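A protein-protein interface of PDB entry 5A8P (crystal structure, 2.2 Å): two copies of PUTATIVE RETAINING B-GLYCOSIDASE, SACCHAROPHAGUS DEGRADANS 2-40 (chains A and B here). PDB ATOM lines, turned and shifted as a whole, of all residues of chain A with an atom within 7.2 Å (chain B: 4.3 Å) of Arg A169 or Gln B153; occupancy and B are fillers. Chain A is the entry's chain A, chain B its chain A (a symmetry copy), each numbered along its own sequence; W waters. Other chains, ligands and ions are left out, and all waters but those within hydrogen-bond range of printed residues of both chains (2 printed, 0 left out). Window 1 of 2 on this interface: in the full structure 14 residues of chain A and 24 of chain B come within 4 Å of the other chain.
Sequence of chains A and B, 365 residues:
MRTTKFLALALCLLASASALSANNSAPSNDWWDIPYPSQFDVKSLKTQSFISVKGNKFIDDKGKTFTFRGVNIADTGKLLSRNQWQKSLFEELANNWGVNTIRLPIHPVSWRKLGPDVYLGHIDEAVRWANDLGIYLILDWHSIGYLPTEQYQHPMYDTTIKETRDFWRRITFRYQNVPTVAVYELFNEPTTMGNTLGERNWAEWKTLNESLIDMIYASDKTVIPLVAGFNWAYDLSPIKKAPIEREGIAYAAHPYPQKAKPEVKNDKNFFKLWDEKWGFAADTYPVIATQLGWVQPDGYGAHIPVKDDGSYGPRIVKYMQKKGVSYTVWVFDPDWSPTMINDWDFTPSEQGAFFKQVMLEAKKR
Water W1 lies within hydrogen-bond range of O of Met A215 (2.8 Å) and O of Thr B196 (2.8 Å). Water W2 lies within hydrogen-bond range of N of Tyr B152 (2.8 Å) and NH1 of Arg A169 (3.5 Å).
Hydrophobic or aromatic side chains of chain A within 4 Å of the printed part of chain B: Tyr A36 and Met A215. Along chain B the printed residues that touch a printed residue of chain A span positions 152 to 197. Among the printed residues, 6 pairs touch across the chains. Among the printed residues, no Asp or Glu carboxylate lies within 4 Å of a Lys or Arg side-chain nitrogen of the other chain.
Printed residues of chain B within 4 Å of Tyr A36: Gln B153 and His B154. Thr A164 touches none of the printed residues of chain B. Of chain B, only Tyr B152 (2.9 Å), Gln B153 (3.9 Å) and Leu B197 (3.5 Å) come within 4 Å of Arg A169. Ile A171 touches none of the printed residues of chain B. Printed residues of chain A within 4 Å of Tyr B152: Arg A169 (2.9 Å). Of the printed residues of chain A, His B154 touches Tyr A36. The nearest residue of chain A that does not touch Gln B153 is Pro A37 (5.7 Å). The nearest printed residue of chain A that does not touch His B154 is Arg A169 (5.1 Å).
O of Met B193 sits at hydrogen-bond distance from OG1 of Thr B196, 2.6 Å away. OE1 of Gln B153 sits at hydrogen-bond distance from NE1 of Trp B232, 2.8 Å away. The backbone carbonyl oxygen (O) of Ile B144 lies within hydrogen-bond range of the backbone NH (N) of Gln B153 (2.9 Å). The guanidinium group of Arg A165 lies within hydrogen-bond range of the side-chain sulfur of Met A215, 3.5 Å away.
Among the printed residues, merely in contact across the chains: Tyr A36 with His B154, Arg A169 with Gln B153, Arg A169 with Leu B197 and Met A215 with Thr B196.
No position is printed for both chains.
OH of Tyr A36 is in hydrogen-bond range of NE2 of Gln B153, at 3.0 Å. The backbone carbonyl oxygen of Tyr B152 lies within hydrogen-bond range of the guanidinium group of Arg A169 (2.9 Å).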
ATOM      1  N   TYR A  36     -31.073 -37.136   0.562  1.00  0.00           N
ATOM      2  CA  TYR A  36     -30.514 -35.791   0.490  1.00  0.00           C
ATOM      3  C   TYR A  36     -28.991 -35.861   0.608  1.00  0.00           C
ATOM      4  O   TYR A  36     -28.467 -36.780   1.220  1.00  0.00           O
ATOM      5  CB  TYR A  36     -31.092 -34.913   1.609  1.00  0.00           C
ATOM      6  CG  TYR A  36     -32.458 -34.372   1.271  1.00  0.00           C
ATOM      7  CD1 TYR A  36     -33.607 -35.098   1.555  1.00  0.00           C
ATOM      8  CD2 TYR A  36     -32.596 -33.140   0.641  1.00  0.00           C
ATOM      9  CE1 TYR A  36     -34.864 -34.602   1.225  1.00  0.00           C
ATOM     10  CE2 TYR A  36     -33.833 -32.643   0.306  1.00  0.00           C
ATOM     11  CZ  TYR A  36     -34.968 -33.375   0.602  1.00  0.00           C
ATOM     12  OH  TYR A  36     -36.199 -32.879   0.256  1.00  0.00           O
ATOM     13  N   PRO A  37     -28.276 -34.883   0.020  1.00  0.00           N
ATOM     14  CA  PRO A  37     -26.817 -34.942  -0.016  1.00  0.00           C
ATOM     15  C   PRO A  37     -26.150 -34.615   1.320  1.00  0.00           C
ATOM     16  O   PRO A  37     -26.748 -33.987   2.199  1.00  0.00           O
ATOM     17  CB  PRO A  37     -26.454 -33.868  -1.047  1.00  0.00           C
ATOM     18  CG  PRO A  37     -27.557 -32.876  -0.927  1.00  0.00           C
ATOM     19  CD  PRO A  37     -28.788 -33.716  -0.716  1.00  0.00           C
ATOM     20  N   GLU A 163     -27.321 -26.337 -15.494  1.00  0.00           N
ATOM     21  CA  GLU A 163     -26.338 -27.335 -15.048  1.00  0.00           C
ATOM     22  C   GLU A 163     -25.157 -26.664 -14.338  1.00  0.00           C
ATOM     23  O   GLU A 163     -24.610 -27.185 -13.350  1.00  0.00           O
ATOM     24  CB  GLU A 163     -25.836 -28.145 -16.246  1.00  0.00           C
ATOM     25  CG  GLU A 163     -24.863 -29.264 -15.898  1.00  0.00           C
ATOM     26  CD  GLU A 163     -24.259 -29.918 -17.134  1.00  0.00           C
ATOM     27  OE1 GLU A 163     -23.563 -29.236 -17.913  1.00  0.00           O
ATOM     28  OE2 GLU A 163     -24.476 -31.121 -17.326  1.00  0.00           O
ATOM     29  N   THR A 164     -24.778 -25.498 -14.847  1.00  0.00           N
ATOM     30  CA  THR A 164     -23.703 -24.719 -14.268  1.00  0.00           C
ATOM     31  C   THR A 164     -24.055 -24.249 -12.856  1.00  0.00           C
ATOM     32  O   THR A 164     -23.255 -24.394 -11.922  1.00  0.00           O
ATOM     33  CB  THR A 164     -23.375 -23.526 -15.170  1.00  0.00           C
ATOM     34  OG1 THR A 164     -22.861 -24.013 -16.416  1.00  0.00           O
ATOM     35  CG2 THR A 164     -22.341 -22.606 -14.506  1.00  0.00           C
ATOM     36  N   ARG A 165     -25.254 -23.709 -12.689  1.00  0.00           N
ATOM     37  CA  ARG A 165     -25.727 -23.353 -11.351  1.00  0.00           C
ATOM     38  C   ARG A 165     -25.771 -24.565 -10.427  1.00  0.00           C
ATOM     39  O   ARG A 165     -25.377 -24.486  -9.271  1.00  0.00           O
ATOM     40  CB  ARG A 165     -27.115 -22.780 -11.413  1.00  0.00           C
ATOM     41  CG  ARG A 165     -27.221 -21.393 -11.989  1.00  0.00           C
ATOM     42  CD  ARG A 165     -28.667 -20.960 -11.848  1.00  0.00           C
ATOM     43  NE  ARG A 165     -28.946 -19.729 -12.549  1.00  0.00           N
ATOM     44  CZ  ARG A 165     -28.605 -18.533 -12.109  1.00  0.00           C
ATOM     45  NH1 ARG A 165     -27.943 -18.389 -10.952  1.00  0.00           N
ATOM     46  NH2 ARG A 165     -28.918 -17.476 -12.834  1.00  0.00           N
ATOM     47  N   ASP A 166     -26.288 -25.676 -10.934  1.00  0.00           N
ATOM     48  CA  ASP A 166     -26.411 -26.883 -10.127  1.00  0.00           C
ATOM     49  C   ASP A 166     -25.035 -27.442  -9.719  1.00  0.00           C
ATOM     50  O   ASP A 166     -24.870 -27.946  -8.608  1.00  0.00           O
ATOM     51  CB  ASP A 166     -27.202 -27.950 -10.880  1.00  0.00           C
ATOM     52  CG  ASP A 166     -27.227 -29.265 -10.147  1.00  0.00           C
ATOM     53  OD1 ASP A 166     -27.912 -29.326  -9.107  1.00  0.00           O
ATOM     54  OD2 ASP A 166     -26.544 -30.218 -10.591  1.00  0.00           O
ATOM     55  N   PHE A 167     -24.061 -27.376 -10.620  1.00  0.00           N
ATOM     56  CA  PHE A 167     -22.694 -27.758 -10.280  1.00  0.00           C
ATOM     57  C   PHE A 167     -22.193 -26.945  -9.073  1.00  0.00           C
ATOM     58  O   PHE A 167     -21.750 -27.508  -8.072  1.00  0.00           O
ATOM     59  CB  PHE A 167     -21.767 -27.554 -11.481  1.00  0.00           C
ATOM     60  CG  PHE A 167     -20.309 -27.781 -11.169  1.00  0.00           C
ATOM     61  CD1 PHE A 167     -19.810 -29.061 -11.042  1.00  0.00           C
ATOM     62  CD2 PHE A 167     -19.441 -26.715 -11.007  1.00  0.00           C
ATOM     63  CE1 PHE A 167     -18.471 -29.284 -10.757  1.00  0.00           C
ATOM     64  CE2 PHE A 167     -18.094 -26.933 -10.716  1.00  0.00           C
ATOM     65  CZ  PHE A 167     -17.611 -28.216 -10.593  1.00  0.00           C
ATOM     66  N   TRP A 168     -22.288 -25.621  -9.159  1.00  0.00           N
ATOM     67  CA  TRP A 168     -21.778 -24.764  -8.106  1.00  0.00           C
ATOM     68  C   TRP A 168     -22.569 -24.911  -6.818  1.00  0.00           C
ATOM     69  O   TRP A 168     -21.996 -24.849  -5.731  1.00  0.00           O
ATOM     70  CB  TRP A 168     -21.683 -23.292  -8.570  1.00  0.00           C
ATOM     71  CG  TRP A 168     -20.560 -23.113  -9.514  1.00  0.00           C
ATOM     72  CD1 TRP A 168     -20.623 -22.705 -10.818  1.00  0.00           C
ATOM     73  CD2 TRP A 168     -19.191 -23.415  -9.252  1.00  0.00           C
ATOM     74  NE1 TRP A 168     -19.365 -22.717 -11.376  1.00  0.00           N
ATOM     75  CE2 TRP A 168     -18.472 -23.159 -10.435  1.00  0.00           C
ATOM     76  CE3 TRP A 168     -18.504 -23.900  -8.135  1.00  0.00           C
ATOM     77  CZ2 TRP A 168     -17.092 -23.351 -10.527  1.00  0.00           C
ATOM     78  CZ3 TRP A 168     -17.123 -24.089  -8.228  1.00  0.00           C
ATOM     79  CH2 TRP A 168     -16.440 -23.824  -9.426  1.00  0.00           C
ATOM     80  N   ARG A 169     -23.873 -25.137  -6.934  1.00  0.00           N
ATOM     81  CA  ARG A 169     -24.713 -25.417  -5.766  1.00  0.00           C
ATOM     82  C   ARG A 169     -24.220 -26.655  -5.027  1.00  0.00           C
ATOM     83  O   ARG A 169     -24.074 -26.647  -3.796  1.00  0.00           O
ATOM     84  CB  ARG A 169     -26.172 -25.618  -6.207  1.00  0.00           C
ATOM     85  CG  ARG A 169     -27.172 -25.880  -5.074  1.00  0.00           C
ATOM     86  CD  ARG A 169     -27.290 -27.359  -4.726  1.00  0.00           C
ATOM     87  NE  ARG A 169     -28.361 -27.631  -3.775  1.00  0.00           N
ATOM     88  CZ  ARG A 169     -29.652 -27.786  -4.081  1.00  0.00           C
ATOM     89  NH1 ARG A 169     -30.091 -27.677  -5.338  1.00  0.00           N
ATOM     90  NH2 ARG A 169     -30.527 -28.036  -3.109  1.00  0.00           N
ATOM     91  N   ARG A 170     -23.999 -27.730  -5.775  1.00  0.00           N
ATOM     92  CA  ARG A 170     -23.529 -28.989  -5.206  1.00  0.00           C
ATOM     93  C   ARG A 170     -22.123 -28.874  -4.598  1.00  0.00           C
ATOM     94  O   ARG A 170     -21.873 -29.345  -3.484  1.00  0.00           O
ATOM     95  CB  ARG A 170     -23.499 -30.065  -6.288  1.00  0.00           C
ATOM     96  CG  ARG A 170     -24.853 -30.564  -6.761  1.00  0.00           C
ATOM     97  CD  ARG A 170     -24.609 -31.640  -7.798  1.00  0.00           C
ATOM     98  NE  ARG A 170     -25.799 -32.132  -8.482  1.00  0.00           N
ATOM     99  CZ  ARG A 170     -26.405 -33.294  -8.229  1.00  0.00           C
ATOM    100  NH1 ARG A 170     -26.003 -34.099  -7.257  1.00  0.00           N
ATOM    101  NH2 ARG A 170     -27.451 -33.637  -8.947  1.00  0.00           N
ATOM    102  N   ILE A 171     -21.209 -28.264  -5.351  1.00  0.00           N
ATOM    103  CA  ILE A 171     -19.828 -28.084  -4.910  1.00  0.00           C
ATOM    104  C   ILE A 171     -19.761 -27.258  -3.627  1.00  0.00           C
ATOM    105  O   ILE A 171     -19.065 -27.622  -2.682  1.00  0.00           O
ATOM    106  CB  ILE A 171     -18.992 -27.386  -6.006  1.00  0.00           C
ATOM    107  CG1 ILE A 171     -18.790 -28.322  -7.195  1.00  0.00           C
ATOM    108  CG2 ILE A 171     -17.636 -26.917  -5.474  1.00  0.00           C
ATOM    109  CD1 ILE A 171     -17.797 -29.434  -6.959  1.00  0.00           C
ATOM    110  N   THR A 172     -20.497 -26.153  -3.593  1.00  0.00           N
ATOM    111  CA  THR A 172     -20.427 -25.244  -2.458  1.00  0.00           C
ATOM    112  C   THR A 172     -20.991 -25.889  -1.182  1.00  0.00           C
ATOM    113  O   THR A 172     -20.427 -25.713  -0.091  1.00  0.00           O
ATOM    114  CB  THR A 172     -21.131 -23.899  -2.746  1.00  0.00           C
ATOM    115  OG1 THR A 172     -20.640 -23.336  -3.966  1.00  0.00           O
ATOM    116  CG2 THR A 172     -20.836 -22.922  -1.629  1.00  0.00           C
ATOM    117  N   PHE A 173     -22.079 -26.647  -1.316  1.00  0.00           N
ATOM    118  CA  PHE A 173     -22.642 -27.379  -0.181  1.00  0.00           C
ATOM    119  C   PHE A 173     -21.655 -28.426   0.337  1.00  0.00           C
ATOM    120  O   PHE A 173     -21.386 -28.503   1.537  1.00  0.00           O
ATOM    121  CB  PHE A 173     -23.960 -28.050  -0.566  1.00  0.00           C
ATOM    122  CG  PHE A 173     -24.563 -28.898   0.522  1.00  0.00           C
ATOM    123  CD1 PHE A 173     -25.225 -28.318   1.603  1.00  0.00           C
ATOM    124  CD2 PHE A 173     -24.519 -30.280   0.438  1.00  0.00           C
ATOM    125  CE1 PHE A 173     -25.794 -29.110   2.596  1.00  0.00           C
ATOM    126  CE2 PHE A 173     -25.085 -31.076   1.418  1.00  0.00           C
ATOM    127  CZ  PHE A 173     -25.724 -30.496   2.498  1.00  0.00           C
ATOM    128  N   ARG A 174     -21.103 -29.213  -0.576  1.00  0.00           N
ATOM    129  CA  ARG A 174     -20.281 -30.341  -0.189  1.00  0.00           C
ATOM    130  C   ARG A 174     -18.980 -29.936   0.490  1.00  0.00           C
ATOM    131  O   ARG A 174     -18.568 -30.599   1.440  1.00  0.00           O
ATOM    132  CB  ARG A 174     -19.945 -31.227  -1.384  1.00  0.00           C
ATOM    133  CG  ARG A 174     -19.477 -32.618  -0.960  1.00  0.00           C
ATOM    134  CD  ARG A 174     -19.065 -33.394  -2.185  1.00  0.00           C
ATOM    135  NE  ARG A 174     -18.663 -34.769  -1.934  1.00  0.00           N
ATOM    136  CZ  ARG A 174     -19.465 -35.823  -2.064  1.00  0.00           C
ATOM    137  NH1 ARG A 174     -20.746 -35.671  -2.391  1.00  0.00           N
ATOM    138  NH2 ARG A 174     -18.982 -37.041  -1.856  1.00  0.00           N
ATOM    139  N   LEU A 212     -24.115 -16.307  -9.947  1.00  0.00           N
ATOM    140  CA  LEU A 212     -23.411 -17.495  -9.443  1.00  0.00           C
ATOM    141  C   LEU A 212     -22.725 -17.194  -8.101  1.00  0.00           C
ATOM    142  O   LEU A 212     -22.813 -17.977  -7.172  1.00  0.00           O
ATOM    143  CB  LEU A 212     -22.384 -17.998 -10.453  1.00  0.00           C
ATOM    144  CG  LEU A 212     -22.943 -18.567 -11.762  1.00  0.00           C
ATOM    145  CD1 LEU A 212     -21.808 -18.929 -12.700  1.00  0.00           C
ATOM    146  CD2 LEU A 212     -23.836 -19.777 -11.523  1.00  0.00           C
ATOM    147  N   MET A 215     -25.238 -17.324  -5.248  1.00  0.00           N
ATOM    148  CA  MET A 215     -25.571 -18.710  -4.868  1.00  0.00           C
ATOM    149  C   MET A 215     -24.488 -19.295  -3.990  1.00  0.00           C
ATOM    150  O   MET A 215     -24.778 -19.966  -3.007  1.00  0.00           O
ATOM    151  CB  MET A 215     -25.708 -19.619  -6.091  1.00  0.00           C
ATOM    152  CG  MET A 215     -26.996 -19.435  -6.864  1.00  0.00           C
ATOM    153  SD  MET A 215     -27.029 -20.536  -8.282  1.00  0.00           S
ATOM    154  CE  MET A 215     -27.304 -22.090  -7.433  1.00  0.00           C
ATOM    155  N   ILE A 216     -23.236 -19.042  -4.369  1.00  0.00           N
ATOM    156  CA  ILE A 216     -22.092 -19.553  -3.638  1.00  0.00           C
ATOM    157  C   ILE A 216     -21.992 -18.936  -2.246  1.00  0.00           C
ATOM    158  O   ILE A 216     -21.867 -19.665  -1.257  1.00  0.00           O
ATOM    159  CB  ILE A 216     -20.788 -19.323  -4.426  1.00  0.00           C
ATOM    160  CG1 ILE A 216     -20.789 -20.217  -5.665  1.00  0.00           C
ATOM    161  CG2 ILE A 216     -19.566 -19.610  -3.569  1.00  0.00           C
ATOM    162  CD1 ILE A 216     -19.695 -19.899  -6.656  1.00  0.00           C
ATOM    163  N   SER A 219     -24.128 -19.983   0.496  1.00  0.00           N
ATOM    164  CA  SER A 219     -23.825 -21.325   1.008  1.00  0.00           C
ATOM    165  C   SER A 219     -22.478 -21.409   1.738  1.00  0.00           C
ATOM    166  O   SER A 219     -22.363 -22.114   2.730  1.00  0.00           O
ATOM    167  CB  SER A 219     -23.881 -22.333  -0.150  1.00  0.00           C
ATOM    168  OG  SER A 219     -23.540 -23.656   0.251  1.00  0.00           O
ATOM    169  N   ILE B 144     -40.410 -28.166  -5.453  1.00  0.00           N
ATOM    170  CA  ILE B 144     -39.958 -27.347  -4.326  1.00  0.00           C
ATOM    171  C   ILE B 144     -38.659 -26.728  -4.771  1.00  0.00           C
ATOM    172  O   ILE B 144     -37.716 -27.446  -5.094  1.00  0.00           O
ATOM    173  CB  ILE B 144     -39.674 -28.173  -3.055  1.00  0.00           C
ATOM    174  CG1 ILE B 144     -40.917 -28.954  -2.631  1.00  0.00           C
ATOM    175  CG2 ILE B 144     -39.187 -27.268  -1.918  1.00  0.00           C
ATOM    176  CD1 ILE B 144     -40.735 -29.738  -1.346  1.00  0.00           C
ATOM    177  N   TYR B 152     -33.620 -26.714  -7.344  1.00  0.00           N
ATOM    178  CA  TYR B 152     -34.640 -27.306  -6.487  1.00  0.00           C
ATOM    179  C   TYR B 152     -34.096 -27.917  -5.214  1.00  0.00           C
ATOM    180  O   TYR B 152     -32.898 -28.133  -5.065  1.00  0.00           O
ATOM    181  CB  TYR B 152     -35.407 -28.363  -7.293  1.00  0.00           C
ATOM    182  CG  TYR B 152     -35.884 -27.775  -8.577  1.00  0.00           C
ATOM    183  CD1 TYR B 152     -37.046 -27.025  -8.623  1.00  0.00           C
ATOM    184  CD2 TYR B 152     -35.109 -27.866  -9.722  1.00  0.00           C
ATOM    185  CE1 TYR B 152     -37.462 -26.432  -9.806  1.00  0.00           C
ATOM    186  CE2 TYR B 152     -35.501 -27.280 -10.891  1.00  0.00           C
ATOM    187  CZ  TYR B 152     -36.681 -26.568 -10.937  1.00  0.00           C
ATOM    188  OH  TYR B 152     -37.074 -25.984 -12.109  1.00  0.00           O
ATOM    189  N   GLN B 153     -35.008 -28.211  -4.298  1.00  0.00           N
ATOM    190  CA  GLN B 153     -34.640 -28.816  -3.028  1.00  0.00           C
ATOM    191  C   GLN B 153     -34.094 -30.251  -3.181  1.00  0.00           C
ATOM    192  O   GLN B 153     -33.286 -30.676  -2.387  1.00  0.00           O
ATOM    193  CB  GLN B 153     -35.840 -28.790  -2.073  1.00  0.00           C
ATOM    194  CG  GLN B 153     -35.609 -29.498  -0.742  1.00  0.00           C
ATOM    195  CD  GLN B 153     -36.635 -29.108   0.313  1.00  0.00           C
ATOM    196  OE1 GLN B 153     -36.897 -27.926   0.533  1.00  0.00           O
ATOM    197  NE2 GLN B 153     -37.220 -30.105   0.972  1.00  0.00           N
ATOM    198  N   HIS B 154     -34.546 -30.982  -4.192  1.00  0.00           N
ATOM    199  CA  HIS B 154     -34.204 -32.398  -4.343  1.00  0.00           C
ATOM    200  C   HIS B 154     -34.538 -32.805  -5.772  1.00  0.00           C
ATOM    201  O   HIS B 154     -35.486 -32.277  -6.349  1.00  0.00           O
ATOM    202  CB  HIS B 154     -35.035 -33.212  -3.335  1.00  0.00           C
ATOM    203  CG  HIS B 154     -34.715 -34.675  -3.286  1.00  0.00           C
ATOM    204  ND1 HIS B 154     -35.147 -35.561  -4.247  1.00  0.00           N
ATOM    205  CD2 HIS B 154     -34.075 -35.421  -2.353  1.00  0.00           C
ATOM    206  CE1 HIS B 154     -34.763 -36.784  -3.929  1.00  0.00           C
ATOM    207  NE2 HIS B 154     -34.112 -36.727  -2.781  1.00  0.00           N
ATOM    208  N   MET B 193     -34.261 -21.497  -0.535  1.00  0.00           N
ATOM    209  CA  MET B 193     -33.464 -22.090   0.543  1.00  0.00           C
ATOM    210  C   MET B 193     -32.344 -21.163   1.032  1.00  0.00           C
ATOM    211  O   MET B 193     -31.162 -21.485   0.938  1.00  0.00           O
ATOM    212  CB  MET B 193     -32.894 -23.450   0.105  1.00  0.00           C
ATOM    213  CG  MET B 193     -33.945 -24.450  -0.368  1.00  0.00           C
ATOM    214  SD  MET B 193     -33.276 -26.070  -0.851  1.00  0.00           S
ATOM    215  CE  MET B 193     -32.917 -26.754   0.758  1.00  0.00           C
ATOM    216  N   THR B 196     -29.703 -19.960  -1.565  1.00  0.00           N
ATOM    217  CA  THR B 196     -28.755 -20.927  -2.119  1.00  0.00           C
ATOM    218  C   THR B 196     -29.161 -21.404  -3.527  1.00  0.00           C
ATOM    219  O   THR B 196     -28.315 -21.854  -4.303  1.00  0.00           O
ATOM    220  CB  THR B 196     -28.592 -22.151  -1.201  1.00  0.00           C
ATOM    221  OG1 THR B 196     -29.868 -22.751  -0.985  1.00  0.00           O
ATOM    222  CG2 THR B 196     -27.982 -21.742   0.150  1.00  0.00           C
ATOM    223  N   LEU B 197     -30.448 -21.301  -3.847  1.00  0.00           N
ATOM    224  CA  LEU B 197     -30.996 -21.744  -5.137  1.00  0.00           C
ATOM    225  C   LEU B 197     -31.112 -20.618  -6.179  1.00  0.00           C
ATOM    226  O   LEU B 197     -31.389 -20.887  -7.349  1.00  0.00           O
ATOM    227  CB  LEU B 197     -32.388 -22.364  -4.931  1.00  0.00           C
ATOM    228  CG  LEU B 197     -32.486 -23.558  -3.997  1.00  0.00           C
ATOM    229  CD1 LEU B 197     -33.882 -24.160  -4.091  1.00  0.00           C
ATOM    230  CD2 LEU B 197     -31.426 -24.614  -4.308  1.00  0.00           C
ATOM    231  N   TRP B 232     -41.396 -21.573   1.110  1.00  0.00           N
ATOM    232  CA  TRP B 232     -42.165 -22.813   0.980  1.00  0.00           C
ATOM    233  C   TRP B 232     -43.671 -22.529   1.008  1.00  0.00           C
ATOM    234  O   TRP B 232     -44.427 -23.174   1.717  1.00  0.00           O
ATOM    235  CB  TRP B 232     -41.757 -23.849   2.047  1.00  0.00           C
ATOM    236  CG  TRP B 232     -40.384 -24.461   1.856  1.00  0.00           C
ATOM    237  CD1 TRP B 232     -40.093 -25.634   1.199  1.00  0.00           C
ATOM    238  CD2 TRP B 232     -39.121 -23.967   2.357  1.00  0.00           C
ATOM    239  NE1 TRP B 232     -38.738 -25.886   1.254  1.00  0.00           N
ATOM    240  CE2 TRP B 232     -38.121 -24.884   1.953  1.00  0.00           C
ATOM    241  CE3 TRP B 232     -38.745 -22.847   3.101  1.00  0.00           C
ATOM    242  CZ2 TRP B 232     -36.760 -24.710   2.270  1.00  0.00           C
ATOM    243  CZ3 TRP B 232     -37.388 -22.664   3.414  1.00  0.00           C
ATOM    244  CH2 TRP B 232     -36.412 -23.598   2.997  1.00  0.00           C
HETATM  245  O   HOH W   1     -25.760 -22.498  -3.472  1.00  0.00           O
HETATM  246  O   HOH W   2     -31.522 -28.311  -8.413  1.00  0.00           O
